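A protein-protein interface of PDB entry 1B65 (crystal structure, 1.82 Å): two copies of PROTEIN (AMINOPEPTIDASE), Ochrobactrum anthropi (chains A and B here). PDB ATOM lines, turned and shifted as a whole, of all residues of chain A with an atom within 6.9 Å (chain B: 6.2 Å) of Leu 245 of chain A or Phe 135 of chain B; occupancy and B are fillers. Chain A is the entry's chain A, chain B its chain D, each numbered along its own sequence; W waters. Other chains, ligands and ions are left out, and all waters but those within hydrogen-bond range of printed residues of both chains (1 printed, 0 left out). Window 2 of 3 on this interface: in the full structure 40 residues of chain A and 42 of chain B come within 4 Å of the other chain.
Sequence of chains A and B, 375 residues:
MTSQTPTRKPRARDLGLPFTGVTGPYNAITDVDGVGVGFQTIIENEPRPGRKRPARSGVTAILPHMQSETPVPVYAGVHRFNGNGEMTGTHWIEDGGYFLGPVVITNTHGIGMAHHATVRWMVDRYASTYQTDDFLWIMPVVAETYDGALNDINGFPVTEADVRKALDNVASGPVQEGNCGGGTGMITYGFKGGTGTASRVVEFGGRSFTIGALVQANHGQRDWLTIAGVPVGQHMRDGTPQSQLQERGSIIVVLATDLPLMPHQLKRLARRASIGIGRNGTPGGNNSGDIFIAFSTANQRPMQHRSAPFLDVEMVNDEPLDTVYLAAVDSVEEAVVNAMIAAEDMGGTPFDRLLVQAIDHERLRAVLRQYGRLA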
ATOM      1  N   ARG A  53     -17.174   4.749  19.709  1.00  0.00           N
ATOM      2  CA  ARG A  53     -17.227   5.856  18.744  1.00  0.00           C
ATOM      3  C   ARG A  53     -18.522   6.618  18.953  1.00  0.00           C
ATOM      4  O   ARG A  53     -19.537   6.050  19.327  1.00  0.00           O
ATOM      5  CB  ARG A  53     -17.176   5.303  17.316  1.00  0.00           C
ATOM      6  CG  ARG A  53     -15.983   4.424  16.974  1.00  0.00           C
ATOM      7  CD  ARG A  53     -16.021   3.931  15.526  1.00  0.00           C
ATOM      8  NE  ARG A  53     -16.143   5.080  14.635  1.00  0.00           N
ATOM      9  CZ  ARG A  53     -16.796   5.061  13.476  1.00  0.00           C
ATOM     10  NH1 ARG A  53     -17.382   3.944  13.047  1.00  0.00           N
ATOM     11  NH2 ARG A  53     -16.820   6.183  12.789  1.00  0.00           N
ATOM     12  N   TYR A 146     -24.060   6.142   3.631  1.00  0.00           N
ATOM     13  CA  TYR A 146     -23.248   5.544   4.698  1.00  0.00           C
ATOM     14  C   TYR A 146     -22.375   6.554   5.454  1.00  0.00           C
ATOM     15  O   TYR A 146     -21.470   7.110   4.858  1.00  0.00           O
ATOM     16  CB  TYR A 146     -22.364   4.492   4.027  1.00  0.00           C
ATOM     17  CG  TYR A 146     -21.371   3.798   4.948  1.00  0.00           C
ATOM     18  CD1 TYR A 146     -21.749   2.771   5.774  1.00  0.00           C
ATOM     19  CD2 TYR A 146     -20.039   4.218   4.896  1.00  0.00           C
ATOM     20  CE1 TYR A 146     -20.801   2.130   6.602  1.00  0.00           C
ATOM     21  CE2 TYR A 146     -19.100   3.593   5.710  1.00  0.00           C
ATOM     22  CZ  TYR A 146     -19.497   2.568   6.545  1.00  0.00           C
ATOM     23  OH  TYR A 146     -18.538   1.940   7.325  1.00  0.00           O
ATOM     24  N   GLY A 148     -20.417   5.759   8.134  1.00  0.00           N
ATOM     25  CA  GLY A 148     -19.535   5.064   9.096  1.00  0.00           C
ATOM     26  C   GLY A 148     -18.198   5.704   9.390  1.00  0.00           C
ATOM     27  O   GLY A 148     -17.608   5.329  10.426  1.00  0.00           O
ATOM     28  N   ALA A 149     -17.699   6.643   8.613  1.00  0.00           N
ATOM     29  CA  ALA A 149     -16.416   7.287   8.927  1.00  0.00           C
ATOM     30  C   ALA A 149     -16.581   8.208  10.117  1.00  0.00           C
ATOM     31  O   ALA A 149     -15.706   8.284  10.998  1.00  0.00           O
ATOM     32  CB  ALA A 149     -15.926   8.042   7.688  1.00  0.00           C
ATOM     33  N   LEU A 150     -17.734   8.895  10.224  1.00  0.00           N
ATOM     34  CA  LEU A 150     -17.941   9.813  11.343  1.00  0.00           C
ATOM     35  C   LEU A 150     -18.952   9.334  12.370  1.00  0.00           C
ATOM     36  O   LEU A 150     -19.055   9.898  13.463  1.00  0.00           O
ATOM     37  CB  LEU A 150     -18.468  11.127  10.726  1.00  0.00           C
ATOM     38  CG  LEU A 150     -17.641  12.381  10.640  1.00  0.00           C
ATOM     39  CD1 LEU A 150     -16.157  12.260  10.912  1.00  0.00           C
ATOM     40  CD2 LEU A 150     -17.945  13.210   9.398  1.00  0.00           C
ATOM     41  N   THR A 240      -7.894  15.864   3.195  1.00  0.00           N
ATOM     42  CA  THR A 240      -8.745  14.775   2.723  1.00  0.00           C
ATOM     43  C   THR A 240      -8.756  13.617   3.705  1.00  0.00           C
ATOM     44  O   THR A 240      -7.758  13.280   4.349  1.00  0.00           O
ATOM     45  CB  THR A 240      -8.318  14.217   1.350  1.00  0.00           C
ATOM     46  OG1 THR A 240      -7.019  13.591   1.483  1.00  0.00           O
ATOM     47  CG2 THR A 240      -8.279  15.307   0.301  1.00  0.00           C
ATOM     48  N   PRO A 241      -9.882  12.923   3.774  1.00  0.00           N
ATOM     49  CA  PRO A 241     -10.040  11.768   4.648  1.00  0.00           C
ATOM     50  C   PRO A 241      -8.949  10.728   4.398  1.00  0.00           C
ATOM     51  O   PRO A 241      -8.373  10.188   5.352  1.00  0.00           O
ATOM     52  CB  PRO A 241     -11.430  11.244   4.313  1.00  0.00           C
ATOM     53  CG  PRO A 241     -12.171  12.475   3.876  1.00  0.00           C
ATOM     54  CD  PRO A 241     -11.149  13.247   3.068  1.00  0.00           C
ATOM     55  N   GLN A 242      -8.635  10.485   3.137  1.00  0.00           N
ATOM     56  CA  GLN A 242      -7.609   9.539   2.721  1.00  0.00           C
ATOM     57  C   GLN A 242      -6.255   9.831   3.346  1.00  0.00           C
ATOM     58  O   GLN A 242      -5.613   8.935   3.904  1.00  0.00           O
ATOM     59  CB  GLN A 242      -7.452   9.564   1.190  1.00  0.00           C
ATOM     60  CG  GLN A 242      -6.650   8.395   0.632  1.00  0.00           C
ATOM     61  CD  GLN A 242      -6.961   8.110  -0.829  1.00  0.00           C
ATOM     62  OE1 GLN A 242      -8.120   7.876  -1.193  1.00  0.00           O
ATOM     63  NE2 GLN A 242      -5.925   8.130  -1.664  1.00  0.00           N
ATOM     64  N   SER A 243      -5.808  11.086   3.283  1.00  0.00           N
ATOM     65  CA  SER A 243      -4.523  11.468   3.853  1.00  0.00           C
ATOM     66  C   SER A 243      -4.450  11.249   5.358  1.00  0.00           C
ATOM     67  O   SER A 243      -3.349  11.049   5.893  1.00  0.00           O
ATOM     68  CB  SER A 243      -4.230  12.923   3.469  1.00  0.00           C
ATOM     69  OG  SER A 243      -5.005  13.794   4.281  1.00  0.00           O
ATOM     70  N   GLN A 244      -5.563  11.272   6.081  1.00  0.00           N
ATOM     71  CA  GLN A 244      -5.563  11.025   7.516  1.00  0.00           C
ATOM     72  C   GLN A 244      -5.576   9.533   7.838  1.00  0.00           C
ATOM     73  O   GLN A 244      -5.065   9.138   8.895  1.00  0.00           O
ATOM     74  CB  GLN A 244      -6.733  11.756   8.188  1.00  0.00           C
ATOM     75  CG  GLN A 244      -6.825  13.224   7.762  1.00  0.00           C
ATOM     76  CD  GLN A 244      -8.101  13.882   8.256  1.00  0.00           C
ATOM     77  OE1 GLN A 244      -8.894  14.433   7.477  1.00  0.00           O
ATOM     78  NE2 GLN A 244      -8.284  13.806   9.559  1.00  0.00           N
ATOM     79  N   LEU A 245      -6.114   8.689   6.969  1.00  0.00           N
ATOM     80  CA  LEU A 245      -6.154   7.245   7.268  1.00  0.00           C
ATOM     81  C   LEU A 245      -5.015   6.479   6.595  1.00  0.00           C
ATOM     82  O   LEU A 245      -4.136   7.034   5.921  1.00  0.00           O
ATOM     83  CB  LEU A 245      -7.498   6.586   6.882  1.00  0.00           C
ATOM     84  CG  LEU A 245      -8.795   7.318   7.450  1.00  0.00           C
ATOM     85  CD1 LEU A 245      -9.982   6.933   6.458  1.00  0.00           C
ATOM     86  CD2 LEU A 245      -9.211   6.508   8.747  1.00  0.00           C
ATOM     87  N   ASN A 287     -18.323   2.400  -5.286  1.00  0.00           N
ATOM     88  CA  ASN A 287     -18.871   2.221  -3.939  1.00  0.00           C
ATOM     89  C   ASN A 287     -19.984   3.206  -3.624  1.00  0.00           C
ATOM     90  O   ASN A 287     -20.566   3.164  -2.520  1.00  0.00           O
ATOM     91  CB  ASN A 287     -17.740   2.387  -2.884  1.00  0.00           C
ATOM     92  CG  ASN A 287     -17.004   1.083  -2.648  1.00  0.00           C
ATOM     93  OD1 ASN A 287     -17.364   0.042  -3.204  1.00  0.00           O
ATOM     94  ND2 ASN A 287     -15.977   1.091  -1.797  1.00  0.00           N
ATOM     95  N   ARG A 353     -11.191   8.972  13.994  1.00  0.00           N
ATOM     96  CA  ARG A 353     -10.057   8.644  13.146  1.00  0.00           C
ATOM     97  C   ARG A 353      -9.760   9.817  12.211  1.00  0.00           C
ATOM     98  O   ARG A 353      -8.690   9.893  11.616  1.00  0.00           O
ATOM     99  CB  ARG A 353     -10.446   7.459  12.254  1.00  0.00           C
ATOM    100  CG  ARG A 353     -10.285   6.128  12.992  1.00  0.00           C
ATOM    101  CD  ARG A 353      -9.813   5.126  11.922  1.00  0.00           C
ATOM    102  NE  ARG A 353     -10.995   4.447  11.417  1.00  0.00           N
ATOM    103  CZ  ARG A 353     -10.941   3.525  10.453  1.00  0.00           C
ATOM    104  NH1 ARG A 353      -9.780   3.202   9.896  1.00  0.00           N
ATOM    105  NH2 ARG A 353     -12.085   2.966  10.087  1.00  0.00           N
ATOM    106  N   LEU A 354     -10.739  10.722  12.059  1.00  0.00           N
ATOM    107  CA  LEU A 354     -10.585  11.819  11.130  1.00  0.00           C
ATOM    108  C   LEU A 354     -11.177  13.125  11.691  1.00  0.00           C
ATOM    109  O   LEU A 354     -12.068  13.069  12.520  1.00  0.00           O
ATOM    110  CB  LEU A 354     -11.373  11.640   9.834  1.00  0.00           C
ATOM    111  CG  LEU A 354     -11.982  10.347   9.343  1.00  0.00           C
ATOM    112  CD1 LEU A 354     -12.985   9.777  10.330  1.00  0.00           C
ATOM    113  CD2 LEU A 354     -12.685  10.551   8.005  1.00  0.00           C
ATOM    114  N   THR B 132     -14.398  -4.385  12.686  1.00  0.00           N
ATOM    115  CA  THR B 132     -13.059  -4.085  12.271  1.00  0.00           C
ATOM    116  C   THR B 132     -12.986  -2.613  11.857  1.00  0.00           C
ATOM    117  O   THR B 132     -13.984  -1.887  11.935  1.00  0.00           O
ATOM    118  CB  THR B 132     -12.626  -4.867  10.999  1.00  0.00           C
ATOM    119  OG1 THR B 132     -13.489  -4.410   9.945  1.00  0.00           O
ATOM    120  CG2 THR B 132     -12.708  -6.370  11.154  1.00  0.00           C
ATOM    121  N   ASP B 133     -11.848  -2.204  11.310  1.00  0.00           N
ATOM    122  CA  ASP B 133     -11.726  -0.814  10.865  1.00  0.00           C
ATOM    123  C   ASP B 133     -12.169  -0.604   9.429  1.00  0.00           C
ATOM    124  O   ASP B 133     -12.233   0.541   8.965  1.00  0.00           O
ATOM    125  CB  ASP B 133     -10.279  -0.324  11.086  1.00  0.00           C
ATOM    126  CG  ASP B 133     -10.252   0.329  12.463  1.00  0.00           C
ATOM    127  OD1 ASP B 133     -10.698  -0.283  13.464  1.00  0.00           O
ATOM    128  OD2 ASP B 133      -9.817   1.500  12.551  1.00  0.00           O
ATOM    129  N   ASP B 134     -12.493  -1.687   8.732  1.00  0.00           N
ATOM    130  CA  ASP B 134     -12.914  -1.604   7.342  1.00  0.00           C
ATOM    131  C   ASP B 134     -14.230  -0.838   7.264  1.00  0.00           C
ATOM    132  O   ASP B 134     -15.081  -0.955   8.134  1.00  0.00           O
ATOM    133  CB  ASP B 134     -13.049  -3.012   6.751  1.00  0.00           C
ATOM    134  CG  ASP B 134     -11.675  -3.692   6.710  1.00  0.00           C
ATOM    135  OD1 ASP B 134     -10.751  -3.012   6.206  1.00  0.00           O
ATOM    136  OD2 ASP B 134     -11.539  -4.846   7.156  1.00  0.00           O
ATOM    137  N   PHE B 135     -14.395  -0.051   6.200  1.00  0.00           N
ATOM    138  CA  PHE B 135     -15.686   0.617   6.022  1.00  0.00           C
ATOM    139  C   PHE B 135     -16.585  -0.308   5.200  1.00  0.00           C
ATOM    140  O   PHE B 135     -16.329  -0.424   4.006  1.00  0.00           O
ATOM    141  CB  PHE B 135     -15.499   1.922   5.250  1.00  0.00           C
ATOM    142  CG  PHE B 135     -14.760   2.920   6.104  1.00  0.00           C
ATOM    143  CD1 PHE B 135     -15.170   3.151   7.402  1.00  0.00           C
ATOM    144  CD2 PHE B 135     -13.668   3.604   5.591  1.00  0.00           C
ATOM    145  CE1 PHE B 135     -14.504   4.061   8.198  1.00  0.00           C
ATOM    146  CE2 PHE B 135     -12.996   4.520   6.394  1.00  0.00           C
ATOM    147  CZ  PHE B 135     -13.415   4.740   7.690  1.00  0.00           C
ATOM    148  N   LEU B 136     -17.470  -0.987   5.885  1.00  0.00           N
ATOM    149  CA  LEU B 136     -18.295  -1.993   5.200  1.00  0.00           C
ATOM    150  C   LEU B 136     -19.746  -1.740   5.546  1.00  0.00           C
ATOM    151  O   LEU B 136     -20.018  -1.237   6.638  1.00  0.00           O
ATOM    152  CB  LEU B 136     -17.910  -3.366   5.779  1.00  0.00           C
ATOM    153  CG  LEU B 136     -16.981  -4.345   5.107  1.00  0.00           C
ATOM    154  CD1 LEU B 136     -16.204  -3.832   3.928  1.00  0.00           C
ATOM    155  CD2 LEU B 136     -16.088  -5.040   6.153  1.00  0.00           C
ATOM    156  N   TRP B 137     -20.649  -1.975   4.624  1.00  0.00           N
ATOM    157  CA  TRP B 137     -22.075  -1.811   4.915  1.00  0.00           C
ATOM    158  C   TRP B 137     -22.800  -3.101   4.468  1.00  0.00           C
ATOM    159  O   TRP B 137     -22.314  -3.819   3.598  1.00  0.00           O
ATOM    160  CB  TRP B 137     -22.691  -0.642   4.166  1.00  0.00           C
ATOM    161  CG  TRP B 137     -22.292  -0.533   2.741  1.00  0.00           C
ATOM    162  CD1 TRP B 137     -22.926  -1.077   1.663  1.00  0.00           C
ATOM    163  CD2 TRP B 137     -21.115   0.109   2.222  1.00  0.00           C
ATOM    164  NE1 TRP B 137     -22.234  -0.797   0.509  1.00  0.00           N
ATOM    165  CE2 TRP B 137     -21.115  -0.064   0.832  1.00  0.00           C
ATOM    166  CE3 TRP B 137     -20.076   0.836   2.821  1.00  0.00           C
ATOM    167  CZ2 TRP B 137     -20.106   0.436   0.011  1.00  0.00           C
ATOM    168  CZ3 TRP B 137     -19.069   1.340   2.000  1.00  0.00           C
ATOM    169  CH2 TRP B 137     -19.091   1.148   0.606  1.00  0.00           C
HETATM  170  O   HOH W   1     -19.229   0.138   9.140  1.00  0.00           O
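Gln 244 of chain A touches none of the printed residues of chain B.
Leu 245 of chain A touches just one residue of chain B: Phe 135.
Thr 132 of chain B touches none of the printed residues of chain A.
Of the printed residues of chain A, Asp 133 of chain B touches Arg 353.
Of the printed residues of chain A, Leu 136 of chain B touches Tyr 146 (3.4 Å).
The nearest printed residue of chain B that does not touch Leu 245 of chain A is Asp 133 of chain B (6.3 Å).
The nearest residue of chain A that does not touch Phe 135 of chain B is Gly 148 of chain A (4.03 Å).
No position is printed for both chains.
Of the 8 pairs that touch across the chains among the printed residues, none has its exchanged pair printed and touching as well.
Of the 6 printed residues of chain B, 4 touch a printed residue of chain A.
Among the printed residues, 8 pairs touch across the chains.
Among the printed residues, Asp or Glu carboxylates within 4 Å of a Lys or Arg side-chain nitrogen of the other chain: Arg 353 of chain A with Asp 133 of chain B (3.2 Å).
Water W1 bridges OH of Tyr 146 of chain A (2.6 Å) and O of Leu 136 of chain B (3.0 Å).
The guanidinium group of Arg 53 of chain A lies within hydrogen-bond range of the backbone carbonyl oxygen of Ala 149 of chain A (3.0 Å).
Among the printed residues, pairs that only touch across the chains: Tyr 146 of chain A with Phe 135 of chain B, Tyr 146 of chain A with Trp 137 of chain B, Ala 149 of chain A with Phe 135 of chain B, Leu 245 of chain A with Phe 135 of chain B, Asn 287 of chain A with Trp 137 of chain B and Arg 353 of chain A with Phe 135 of chain B.
OD2 of Asp 133 of chain B is in salt-bridge range of NH1 of Arg 353 of chain A.
The side-chain hydroxyl (OH) of Tyr 146 of chain A is in hydrogen-bond range of the backbone NH (N) of Leu 136 of chain B (3.4 Å).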
